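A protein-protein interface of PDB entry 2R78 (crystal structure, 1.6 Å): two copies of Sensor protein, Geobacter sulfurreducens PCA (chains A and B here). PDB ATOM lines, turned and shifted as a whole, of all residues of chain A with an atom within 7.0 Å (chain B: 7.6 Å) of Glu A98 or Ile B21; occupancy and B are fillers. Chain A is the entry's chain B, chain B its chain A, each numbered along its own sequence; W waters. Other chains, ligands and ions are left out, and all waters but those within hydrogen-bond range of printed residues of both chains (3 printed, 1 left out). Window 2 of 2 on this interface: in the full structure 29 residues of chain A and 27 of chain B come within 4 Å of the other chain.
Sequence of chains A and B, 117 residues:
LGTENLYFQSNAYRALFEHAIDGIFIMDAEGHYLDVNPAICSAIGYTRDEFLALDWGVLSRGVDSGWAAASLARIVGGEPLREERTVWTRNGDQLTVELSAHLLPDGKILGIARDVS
Among the printed residues, merely in contact across the chains: Asp A22 with Asp B22, Arg A82 with Ile B21, Glu A98 with Ile B21, Ile A112 with Leu B16, Arg A114 with Ile B21 and Arg A114 with Arg B114.
Hydrophobic or aromatic side chains of chain A within 4 Å of the printed part of chain B: Ile A112.
Of the 17 printed residues of chain B, 4 touch a printed residue of chain A.
Printed residues of chain B that touch a printed residue of chain A: Leu B16, Ile B21, Asp B22 and Arg B114.
Hydrophobic or aromatic side chains of chain B within 4 Å of the printed part of chain A: Leu B16 and Ile B21.
O of Asp B22 lies within hydrogen-bond range of ND2 of Asn B37.
OD2 of Asp B22 is in salt-bridge range of NH1 of Arg B114 (2.7 Å).
OD2 of Asp A22 lies within salt-bridge range of NH1 of Arg A114 (2.6 Å).
The guanidinium group (NE) of Arg A82 sits at hydrogen-bond distance from the side-chain hydroxyl (OG) of Ser A100 (2.5 Å).
The backbone NH (N) of Glu A98 sits at hydrogen-bond distance from the backbone carbonyl oxygen (O) of Arg A114 (2.8 Å).
N of Ile A112 sits at hydrogen-bond distance from O of Ser A100.
Water W3 lies within hydrogen-bond range of the side-chain carboxylate of Asp A22, the backbone NH of Asp B22 and the guanidinium group of Arg A114.
Water W1 bridges O of His B19 (2.7 Å) and NH2 of Arg A82 (3.3 Å).
Water W2 lies within hydrogen-bond range of O of His B19, NH2 of Arg A82 and OG of Ser A100.
Of the printed residues of chain B, Arg A82 touches Ile B21.
Printed residues of chain B within 4 Å of Glu A98: Ile B21 (3.5 Å).
Printed residues of chain B within 4 Å of Arg A114: Ile B21 (3.6 Å), Asp B22 (2.9 Å) and Arg B114 (3.97 Å).
Ala B20 touches none of the printed residues of chain A.
Ile B21 touches three residues of chain A.
Printed residues of chain A within 4 Å of Asp B22: Asp A22 (3.7 Å) and Arg A114 (2.9 Å).
Of the printed residues of chain A, Arg B114 touches Asp A22 (2.9 Å) and Arg A114 (3.97 Å).
The nearest printed residue of chain B that does not touch Arg A82 is His B19 (4.3 Å).
Asp B22 touches its own counterpart, Asp A22.
Asp A22 touches Arg B114, and with the chains exchanged Arg A114 touches Asp B22.
Arg A114 touches its own counterpart, Arg B114.
Of the 8 pairs that touch across the chains among the printed residues, 4 have their exchanged pair printed and touching as well.
OD1 of Asp B22 lies within salt-bridge range of NH1 of Arg A114 (2.9 Å).
The side-chain carboxylate of Asp A22 lies within salt-bridge range of the guanidinium group of Arg B114 (2.9 Å).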
ATOM      1  N   ASP A  22      28.350   6.612  26.818  1.00  0.00           N
ATOM      2  CA  ASP A  22      28.584   5.608  27.850  1.00  0.00           C
ATOM      3  C   ASP A  22      29.851   5.916  28.652  1.00  0.00           C
ATOM      4  O   ASP A  22      30.803   6.536  28.154  1.00  0.00           O
ATOM      5  CB  ASP A  22      28.709   4.224  27.264  1.00  0.00           C
ATOM      6  CG  ASP A  22      27.382   3.650  26.810  1.00  0.00           C
ATOM      7  OD1 ASP A  22      26.285   4.140  27.202  1.00  0.00           O
ATOM      8  OD2 ASP A  22      27.458   2.661  26.077  1.00  0.00           O
ATOM      9  N   LEU A  81      33.236  -9.676  32.108  1.00  0.00           N
ATOM     10  CA  LEU A  81      32.165  -9.361  33.012  1.00  0.00           C
ATOM     11  C   LEU A  81      31.069  -8.698  32.208  1.00  0.00           C
ATOM     12  O   LEU A  81      31.337  -7.855  31.338  1.00  0.00           O
ATOM     13  CB  LEU A  81      32.684  -8.429  34.107  1.00  0.00           C
ATOM     14  CG  LEU A  81      31.670  -7.917  35.125  1.00  0.00           C
ATOM     15  CD1 LEU A  81      32.306  -7.751  36.519  1.00  0.00           C
ATOM     16  CD2 LEU A  81      31.005  -6.666  34.667  1.00  0.00           C
ATOM     17  N   ARG A  82      29.831  -9.091  32.495  1.00  0.00           N
ATOM     18  CA  ARG A  82      28.664  -8.386  32.024  1.00  0.00           C
ATOM     19  C   ARG A  82      27.589  -8.574  33.067  1.00  0.00           C
ATOM     20  O   ARG A  82      26.972  -9.651  33.157  1.00  0.00           O
ATOM     21  CB  ARG A  82      28.173  -8.936  30.697  1.00  0.00           C
ATOM     22  CG  ARG A  82      26.869  -8.350  30.235  1.00  0.00           C
ATOM     23  CD  ARG A  82      26.998  -6.913  29.800  1.00  0.00           C
ATOM     24  NE  ARG A  82      27.944  -6.792  28.685  1.00  0.00           N
ATOM     25  CZ  ARG A  82      27.643  -6.801  27.385  1.00  0.00           C
ATOM     26  NH1 ARG A  82      26.389  -6.945  26.944  1.00  0.00           N
ATOM     27  NH2 ARG A  82      28.628  -6.678  26.507  1.00  0.00           N
ATOM     28  N   GLU A  83      27.428  -7.551  33.880  1.00  0.00           N
ATOM     29  CA  GLU A  83      26.410  -7.574  34.900  1.00  0.00           C
ATOM     30  C   GLU A  83      26.086  -6.180  35.397  1.00  0.00           C
ATOM     31  O   GLU A  83      26.853  -5.213  35.167  1.00  0.00           O
ATOM     32  CB  GLU A  83      26.853  -8.488  36.039  1.00  0.00           C
ATOM     33  CG  GLU A  83      27.983  -8.010  36.858  1.00  0.00           C
ATOM     34  CD  GLU A  83      28.555  -9.125  37.770  1.00  0.00           C
ATOM     35  OE1 GLU A  83      28.184  -9.172  38.973  1.00  0.00           O
ATOM     36  OE2 GLU A  83      29.332  -9.990  37.262  1.00  0.00           O
ATOM     37  N   GLU A  84      24.932  -6.071  36.048  1.00  0.00           N
ATOM     38  CA  GLU A  84      24.477  -4.808  36.561  1.00  0.00           C
ATOM     39  C   GLU A  84      24.995  -4.608  37.972  1.00  0.00           C
ATOM     40  O   GLU A  84      25.088  -5.558  38.765  1.00  0.00           O
ATOM     41  CB  GLU A  84      22.961  -4.773  36.551  1.00  0.00           C
ATOM     42  CG  GLU A  84      22.364  -4.853  35.149  1.00  0.00           C
ATOM     43  CD  GLU A  84      20.869  -4.705  35.127  1.00  0.00           C
ATOM     44  OE1 GLU A  84      20.282  -4.589  36.234  1.00  0.00           O
ATOM     45  OE2 GLU A  84      20.295  -4.775  34.004  1.00  0.00           O
ATOM     46  N   ARG A  85      25.299  -3.354  38.289  1.00  0.00           N
ATOM     47  CA  ARG A  85      25.681  -2.978  39.627  1.00  0.00           C
ATOM     48  C   ARG A  85      25.025  -1.661  40.024  1.00  0.00           C
ATOM     49  O   ARG A  85      24.938  -0.755  39.216  1.00  0.00           O
ATOM     50  CB  ARG A  85      27.197  -2.822  39.725  1.00  0.00           C
ATOM     51  CG  ARG A  85      27.911  -4.111  39.552  1.00  0.00           C
ATOM     52  CD  ARG A  85      27.680  -5.043  40.690  1.00  0.00           C
ATOM     53  NE  ARG A  85      28.360  -4.689  41.949  1.00  0.00           N
ATOM     54  CZ  ARG A  85      28.228  -5.387  43.070  1.00  0.00           C
ATOM     55  NH1 ARG A  85      27.438  -6.481  43.102  1.00  0.00           N
ATOM     56  NH2 ARG A  85      28.877  -5.040  44.158  1.00  0.00           N
ATOM     57  N   THR A  96      21.893   2.726  38.948  1.00  0.00           N
ATOM     58  CA  THR A  96      22.128   1.343  38.514  1.00  0.00           C
ATOM     59  C   THR A  96      22.653   1.386  37.093  1.00  0.00           C
ATOM     60  O   THR A  96      22.107   2.070  36.220  1.00  0.00           O
ATOM     61  CB  THR A  96      20.887   0.461  38.634  1.00  0.00           C
ATOM     62  OG1 THR A  96      20.511   0.428  40.018  1.00  0.00           O
ATOM     63  CG2 THR A  96      21.176  -0.940  38.186  1.00  0.00           C
ATOM     64  N   VAL A  97      23.758   0.699  36.913  1.00  0.00           N
ATOM     65  CA  VAL A  97      24.409   0.622  35.623  1.00  0.00           C
ATOM     66  C   VAL A  97      24.661  -0.794  35.202  1.00  0.00           C
ATOM     67  O   VAL A  97      24.725  -1.713  36.038  1.00  0.00           O
ATOM     68  CB  VAL A  97      25.724   1.392  35.587  1.00  0.00           C
ATOM     69  CG1 VAL A  97      25.466   2.878  35.908  1.00  0.00           C
ATOM     70  CG2 VAL A  97      26.754   0.794  36.544  1.00  0.00           C
ATOM     71  N   GLU A  98      24.736  -1.001  33.887  1.00  0.00           N
ATOM     72  CA  GLU A  98      25.197  -2.270  33.381  1.00  0.00           C
ATOM     73  C   GLU A  98      26.668  -2.133  33.062  1.00  0.00           C
ATOM     74  O   GLU A  98      27.047  -1.266  32.257  1.00  0.00           O
ATOM     75  CB  GLU A  98      24.479  -2.666  32.113  1.00  0.00           C
ATOM     76  CG  GLU A  98      24.870  -4.049  31.679  1.00  0.00           C
ATOM     77  CD  GLU A  98      24.314  -4.400  30.328  1.00  0.00           C
ATOM     78  OE1 GLU A  98      24.824  -3.855  29.315  1.00  0.00           O
ATOM     79  OE2 GLU A  98      23.368  -5.215  30.296  1.00  0.00           O
ATOM     80  N   LEU A  99      27.470  -3.006  33.656  1.00  0.00           N
ATOM     81  CA  LEU A  99      28.907  -2.977  33.464  1.00  0.00           C
ATOM     82  C   LEU A  99      29.339  -4.083  32.499  1.00  0.00           C
ATOM     83  O   LEU A  99      28.869  -5.212  32.601  1.00  0.00           O
ATOM     84  CB  LEU A  99      29.631  -3.171  34.798  1.00  0.00           C
ATOM     85  CG  LEU A  99      29.388  -2.183  35.934  1.00  0.00           C
ATOM     86  CD1 LEU A  99      30.134  -2.682  37.214  1.00  0.00           C
ATOM     87  CD2 LEU A  99      29.812  -0.764  35.582  1.00  0.00           C
ATOM     88  N   SER A 100      30.286  -3.759  31.629  1.00  0.00           N
ATOM     89  CA  SER A 100      31.021  -4.739  30.853  1.00  0.00           C
ATOM     90  C   SER A 100      32.492  -4.508  31.170  1.00  0.00           C
ATOM     91  O   SER A 100      32.909  -3.358  31.383  1.00  0.00           O
ATOM     92  CB  SER A 100      30.712  -4.533  29.377  1.00  0.00           C
ATOM     93  OG  SER A 100      29.302  -4.728  29.210  1.00  0.00           O
ATOM     94  N   ILE A 112      33.118  -0.644  30.553  1.00  0.00           N
ATOM     95  CA  ILE A 112      32.097   0.237  30.006  1.00  0.00           C
ATOM     96  C   ILE A 112      30.907   0.198  30.987  1.00  0.00           C
ATOM     97  O   ILE A 112      30.559  -0.869  31.482  1.00  0.00           O
ATOM     98  CB  ILE A 112      31.641  -0.251  28.615  1.00  0.00           C
ATOM     99  CG1 ILE A 112      32.802  -0.303  27.608  1.00  0.00           C
ATOM    100  CG2 ILE A 112      30.612   0.687  28.048  1.00  0.00           C
ATOM    101  CD1 ILE A 112      32.469  -1.101  26.301  1.00  0.00           C
ATOM    102  N   ALA A 113      30.325   1.360  31.286  1.00  0.00           N
ATOM    103  CA  ALA A 113      29.151   1.463  32.196  1.00  0.00           C
ATOM    104  C   ALA A 113      28.040   2.133  31.407  1.00  0.00           C
ATOM    105  O   ALA A 113      28.255   3.203  30.863  1.00  0.00           O
ATOM    106  CB  ALA A 113      29.497   2.306  33.429  1.00  0.00           C
ATOM    107  N   ARG A 114      26.862   1.516  31.366  1.00  0.00           N
ATOM    108  CA  ARG A 114      25.701   2.028  30.651  1.00  0.00           C
ATOM    109  C   ARG A 114      24.519   2.202  31.611  1.00  0.00           C
ATOM    110  O   ARG A 114      24.322   1.405  32.535  1.00  0.00           O
ATOM    111  CB  ARG A 114      25.258   1.036  29.563  1.00  0.00           C
ATOM    112  CG  ARG A 114      26.279   0.749  28.460  1.00  0.00           C
ATOM    113  CD  ARG A 114      25.795  -0.264  27.384  1.00  0.00           C
ATOM    114  NE  ARG A 114      24.488   0.080  26.772  1.00  0.00           N
ATOM    115  CZ  ARG A 114      24.307   0.878  25.704  1.00  0.00           C
ATOM    116  NH1 ARG A 114      25.332   1.480  25.118  1.00  0.00           N
ATOM    117  NH2 ARG A 114      23.083   1.112  25.240  1.00  0.00           N
ATOM    118  N   ASP A 115      23.682   3.200  31.373  1.00  0.00           N
ATOM    119  CA  ASP A 115      22.383   3.248  32.094  1.00  0.00           C
ATOM    120  C   ASP A 115      21.476   2.056  31.816  1.00  0.00           C
ATOM    121  O   ASP A 115      21.505   1.506  30.704  1.00  0.00           O
ATOM    122  CB  ASP A 115      21.633   4.522  31.752  1.00  0.00           C
ATOM    123  CG  ASP A 115      22.167   5.706  32.514  1.00  0.00           C
ATOM    124  OD1 ASP A 115      22.240   5.601  33.772  1.00  0.00           O
ATOM    125  OD2 ASP A 115      22.507   6.728  31.860  1.00  0.00           O
ATOM    126  N   VAL A 116      20.671   1.671  32.827  1.00  0.00           N
ATOM    127  CA  VAL A 116      19.835   0.451  32.779  1.00  0.00           C
ATOM    128  C   VAL A 116      18.695   0.427  33.799  1.00  0.00           C
ATOM    129  O   VAL A 116      18.897   0.479  35.025  1.00  0.00           O
ATOM    130  CB  VAL A 116      20.649  -0.818  33.073  1.00  0.00           C
ATOM    131  CG1 VAL A 116      21.989  -0.787  32.313  1.00  0.00           C
ATOM    132  CG2 VAL A 116      20.868  -0.975  34.537  1.00  0.00           C
ATOM    133  N   LEU B  16      36.859  -1.598  22.511  1.00  0.00           N
ATOM    134  CA  LEU B  16      35.643  -0.765  22.508  1.00  0.00           C
ATOM    135  C   LEU B  16      34.847  -0.990  21.230  1.00  0.00           C
ATOM    136  O   LEU B  16      33.637  -1.184  21.259  1.00  0.00           O
ATOM    137  CB  LEU B  16      35.960   0.712  22.626  1.00  0.00           C
ATOM    138  CG  LEU B  16      36.408   1.212  23.991  1.00  0.00           C
ATOM    139  CD1 LEU B  16      37.179   2.532  23.907  1.00  0.00           C
ATOM    140  CD2 LEU B  16      35.171   1.331  24.930  1.00  0.00           C
ATOM    141  N   PHE B  17      35.542  -0.981  20.108  1.00  0.00           N
ATOM    142  CA  PHE B  17      34.874  -1.109  18.822  1.00  0.00           C
ATOM    143  C   PHE B  17      34.140  -2.469  18.772  1.00  0.00           C
ATOM    144  O   PHE B  17      32.980  -2.533  18.415  1.00  0.00           O
ATOM    145  CB  PHE B  17      35.924  -0.990  17.721  1.00  0.00           C
ATOM    146  CG  PHE B  17      35.361  -0.794  16.358  1.00  0.00           C
ATOM    147  CD1 PHE B  17      34.949   0.471  15.943  1.00  0.00           C
ATOM    148  CD2 PHE B  17      35.295  -1.857  15.458  1.00  0.00           C
ATOM    149  CE1 PHE B  17      34.487   0.660  14.651  1.00  0.00           C
ATOM    150  CE2 PHE B  17      34.821  -1.657  14.165  1.00  0.00           C
ATOM    151  CZ  PHE B  17      34.414  -0.420  13.781  1.00  0.00           C
ATOM    152  N   GLU B  18      34.830  -3.534  19.156  1.00  0.00           N
ATOM    153  CA  GLU B  18      34.291  -4.883  19.039  1.00  0.00           C
ATOM    154  C   GLU B  18      33.129  -5.059  19.995  1.00  0.00           C
ATOM    155  O   GLU B  18      32.107  -5.647  19.616  1.00  0.00           O
ATOM    156  CB  GLU B  18      35.377  -5.925  19.345  1.00  0.00           C
ATOM    157  CG  GLU B  18      34.842  -7.357  19.501  1.00  0.00           C
ATOM    158  CD  GLU B  18      34.483  -8.074  18.177  1.00  0.00           C
ATOM    159  OE1 GLU B  18      34.992  -7.729  17.065  1.00  0.00           O
ATOM    160  OE2 GLU B  18      33.681  -9.040  18.266  1.00  0.00           O
ATOM    161  N   HIS B  19      33.286  -4.591  21.231  1.00  0.00           N
ATOM    162  CA  HIS B  19      32.321  -4.949  22.302  1.00  0.00           C
ATOM    163  C   HIS B  19      31.258  -3.912  22.628  1.00  0.00           C
ATOM    164  O   HIS B  19      30.333  -4.202  23.377  1.00  0.00           O
ATOM    165  CB  HIS B  19      33.040  -5.342  23.600  1.00  0.00           C
ATOM    166  CG  HIS B  19      33.951  -6.512  23.429  1.00  0.00           C
ATOM    167  ND1 HIS B  19      33.489  -7.779  23.136  1.00  0.00           N
ATOM    168  CD2 HIS B  19      35.301  -6.599  23.461  1.00  0.00           C
ATOM    169  CE1 HIS B  19      34.521  -8.592  23.003  1.00  0.00           C
ATOM    170  NE2 HIS B  19      35.628  -7.904  23.198  1.00  0.00           N
ATOM    171  N   ALA B  20      31.361  -2.720  22.057  1.00  0.00           N
ATOM    172  CA  ALA B  20      30.393  -1.679  22.338  1.00  0.00           C
ATOM    173  C   ALA B  20      28.996  -2.146  21.985  1.00  0.00           C
ATOM    174  O   ALA B  20      28.793  -2.767  20.946  1.00  0.00           O
ATOM    175  CB  ALA B  20      30.731  -0.383  21.575  1.00  0.00           C
ATOM    176  N   ILE B  21      28.013  -1.778  22.809  1.00  0.00           N
ATOM    177  CA  ILE B  21      26.612  -2.021  22.479  1.00  0.00           C
ATOM    178  C   ILE B  21      26.080  -0.977  21.487  1.00  0.00           C
ATOM    179  O   ILE B  21      25.244  -1.305  20.609  1.00  0.00           O
ATOM    180  CB  ILE B  21      25.780  -2.085  23.761  1.00  0.00           C
ATOM    181  CG1 ILE B  21      26.135  -3.380  24.499  1.00  0.00           C
ATOM    182  CG2 ILE B  21      24.303  -1.991  23.443  1.00  0.00           C
ATOM    183  CD1 ILE B  21      25.513  -3.501  25.916  1.00  0.00           C
ATOM    184  N   ASP B  22      26.563   0.265  21.625  1.00  0.00           N
ATOM    185  CA  ASP B  22      26.298   1.327  20.641  1.00  0.00           C
ATOM    186  C   ASP B  22      26.980   1.011  19.309  1.00  0.00           C
ATOM    187  O   ASP B  22      28.008   0.351  19.262  1.00  0.00           O
ATOM    188  CB  ASP B  22      26.834   2.692  21.117  1.00  0.00           C
ATOM    189  CG  ASP B  22      26.049   3.298  22.280  1.00  0.00           C
ATOM    190  OD1 ASP B  22      24.909   2.842  22.581  1.00  0.00           O
ATOM    191  OD2 ASP B  22      26.585   4.279  22.865  1.00  0.00           O
ATOM    192  N   GLY B  23      26.390   1.504  18.232  1.00  0.00           N
ATOM    193  CA  GLY B  23      27.029   1.435  16.930  1.00  0.00           C
ATOM    194  C   GLY B  23      28.171   2.442  16.875  1.00  0.00           C
ATOM    195  O   GLY B  23      28.079   3.535  17.448  1.00  0.00           O
ATOM    196  N   ILE B  24      29.268   2.035  16.253  1.00  0.00           N
ATOM    197  CA  ILE B  24      30.427   2.904  16.050  1.00  0.00           C
ATOM    198  C   ILE B  24      30.836   2.740  14.603  1.00  0.00           C
ATOM    199  O   ILE B  24      30.925   1.613  14.062  1.00  0.00           O
ATOM    200  CB  ILE B  24      31.628   2.527  16.937  1.00  0.00           C
ATOM    201  CG1 ILE B  24      31.232   2.517  18.426  1.00  0.00           C
ATOM    202  CG2 ILE B  24      32.874   3.427  16.613  1.00  0.00           C
ATOM    203  CD1 ILE B  24      32.296   1.954  19.362  1.00  0.00           C
ATOM    204  N   ASN B  37      31.234  -1.223  13.260  1.00  0.00           N
ATOM    205  CA  ASN B  37      31.443  -2.260  14.265  1.00  0.00           C
ATOM    206  C   ASN B  37      30.337  -3.319  14.261  1.00  0.00           C
ATOM    207  O   ASN B  37      29.315  -3.170  13.594  1.00  0.00           O
ATOM    208  CB  ASN B  37      31.650  -1.640  15.671  1.00  0.00           C
ATOM    209  CG  ASN B  37      30.357  -1.164  16.330  1.00  0.00           C
ATOM    210  OD1 ASN B  37      29.313  -0.917  15.674  1.00  0.00           O
ATOM    211  ND2 ASN B  37      30.426  -1.031  17.670  1.00  0.00           N
ATOM    212  N   PRO B  38      30.546  -4.408  15.011  1.00  0.00           N
ATOM    213  CA  PRO B  38      29.496  -5.436  14.975  1.00  0.00           C
ATOM    214  C   PRO B  38      28.094  -4.957  15.355  1.00  0.00           C
ATOM    215  O   PRO B  38      27.120  -5.362  14.715  1.00  0.00           O
ATOM    216  CB  PRO B  38      30.062  -6.500  15.933  1.00  0.00           C
ATOM    217  CG  PRO B  38      31.521  -6.364  15.797  1.00  0.00           C
ATOM    218  CD  PRO B  38      31.706  -4.864  15.788  1.00  0.00           C
ATOM    219  N   ALA B  39      27.979  -4.126  16.402  1.00  0.00           N
ATOM    220  CA  ALA B  39      26.675  -3.620  16.854  1.00  0.00           C
ATOM    221  C   ALA B  39      25.903  -2.930  15.725  1.00  0.00           C
ATOM    222  O   ALA B  39      24.725  -3.207  15.506  1.00  0.00           O
ATOM    223  CB  ALA B  39      26.829  -2.676  18.048  1.00  0.00           C
ATOM    224  N   ILE B  40      26.579  -2.056  14.979  1.00  0.00           N
ATOM    225  CA  ILE B  40      25.883  -1.306  13.932  1.00  0.00           C
ATOM    226  C   ILE B  40      25.511  -2.205  12.739  1.00  0.00           C
ATOM    227  O   ILE B  40      24.441  -2.050  12.195  1.00  0.00           O
ATOM    228  CB  ILE B  40      26.639  -0.013  13.515  1.00  0.00           C
ATOM    229  CG1 ILE B  40      25.668   1.012  12.900  1.00  0.00           C
ATOM    230  CG2 ILE B  40      27.803  -0.351  12.582  1.00  0.00           C
ATOM    231  CD1 ILE B  40      26.343   2.399  12.634  1.00  0.00           C
ATOM    232  N   ALA B  43      22.403  -4.152  14.027  1.00  0.00           N
ATOM    233  CA  ALA B  43      21.211  -3.300  14.137  1.00  0.00           C
ATOM    234  C   ALA B  43      20.623  -2.942  12.771  1.00  0.00           C
ATOM    235  O   ALA B  43      19.408  -3.035  12.560  1.00  0.00           O
ATOM    236  CB  ALA B  43      21.522  -2.028  14.909  1.00  0.00           C
ATOM    237  N   ALA B 113      26.225   5.613  16.974  1.00  0.00           N
ATOM    238  CA  ALA B 113      24.780   5.489  16.739  1.00  0.00           C
ATOM    239  C   ALA B 113      24.176   4.809  17.969  1.00  0.00           C
ATOM    240  O   ALA B 113      24.621   3.733  18.344  1.00  0.00           O
ATOM    241  CB  ALA B 113      24.545   4.683  15.471  1.00  0.00           C
ATOM    242  N   ARG B 114      23.269   5.492  18.651  1.00  0.00           N
ATOM    243  CA  ARG B 114      22.660   4.957  19.883  1.00  0.00           C
ATOM    244  C   ARG B 114      21.152   4.909  19.748  1.00  0.00           C
ATOM    245  O   ARG B 114      20.572   5.779  19.114  1.00  0.00           O
ATOM    246  CB  ARG B 114      22.975   5.872  21.065  1.00  0.00           C
ATOM    247  CG  ARG B 114      24.443   6.200  21.265  1.00  0.00           C
ATOM    248  CD  ARG B 114      24.703   7.094  22.504  1.00  0.00           C
ATOM    249  NE  ARG B 114      23.780   6.860  23.615  1.00  0.00           N
ATOM    250  CZ  ARG B 114      24.014   6.103  24.694  1.00  0.00           C
ATOM    251  NH1 ARG B 114      25.158   5.442  24.878  1.00  0.00           N
ATOM    252  NH2 ARG B 114      23.067   6.006  25.617  1.00  0.00           N
ATOM    253  N   ASP B 115      20.512   3.927  20.384  1.00  0.00           N
ATOM    254  CA  ASP B 115      19.022   3.944  20.527  1.00  0.00           C
ATOM    255  C   ASP B 115      18.517   5.132  21.357  1.00  0.00           C
ATOM    256  O   ASP B 115      17.442   5.696  21.070  1.00  0.00           O
ATOM    257  CB  ASP B 115      18.526   2.644  21.163  1.00  0.00           C
ATOM    258  CG  ASP B 115      18.719   1.446  20.258  1.00  0.00           C
ATOM    259  OD1 ASP B 115      18.189   1.466  19.112  1.00  0.00           O
ATOM    260  OD2 ASP B 115      19.407   0.484  20.706  1.00  0.00           O
HETATM  261  O   HOH W   1      28.875  -6.430  23.181  1.00  0.00           O
HETATM  262  O   HOH W   2      30.241  -4.299  26.164  1.00  0.00           O
HETATM  263  O   HOH W   3      28.443   1.659  23.812  1.00  0.00           O
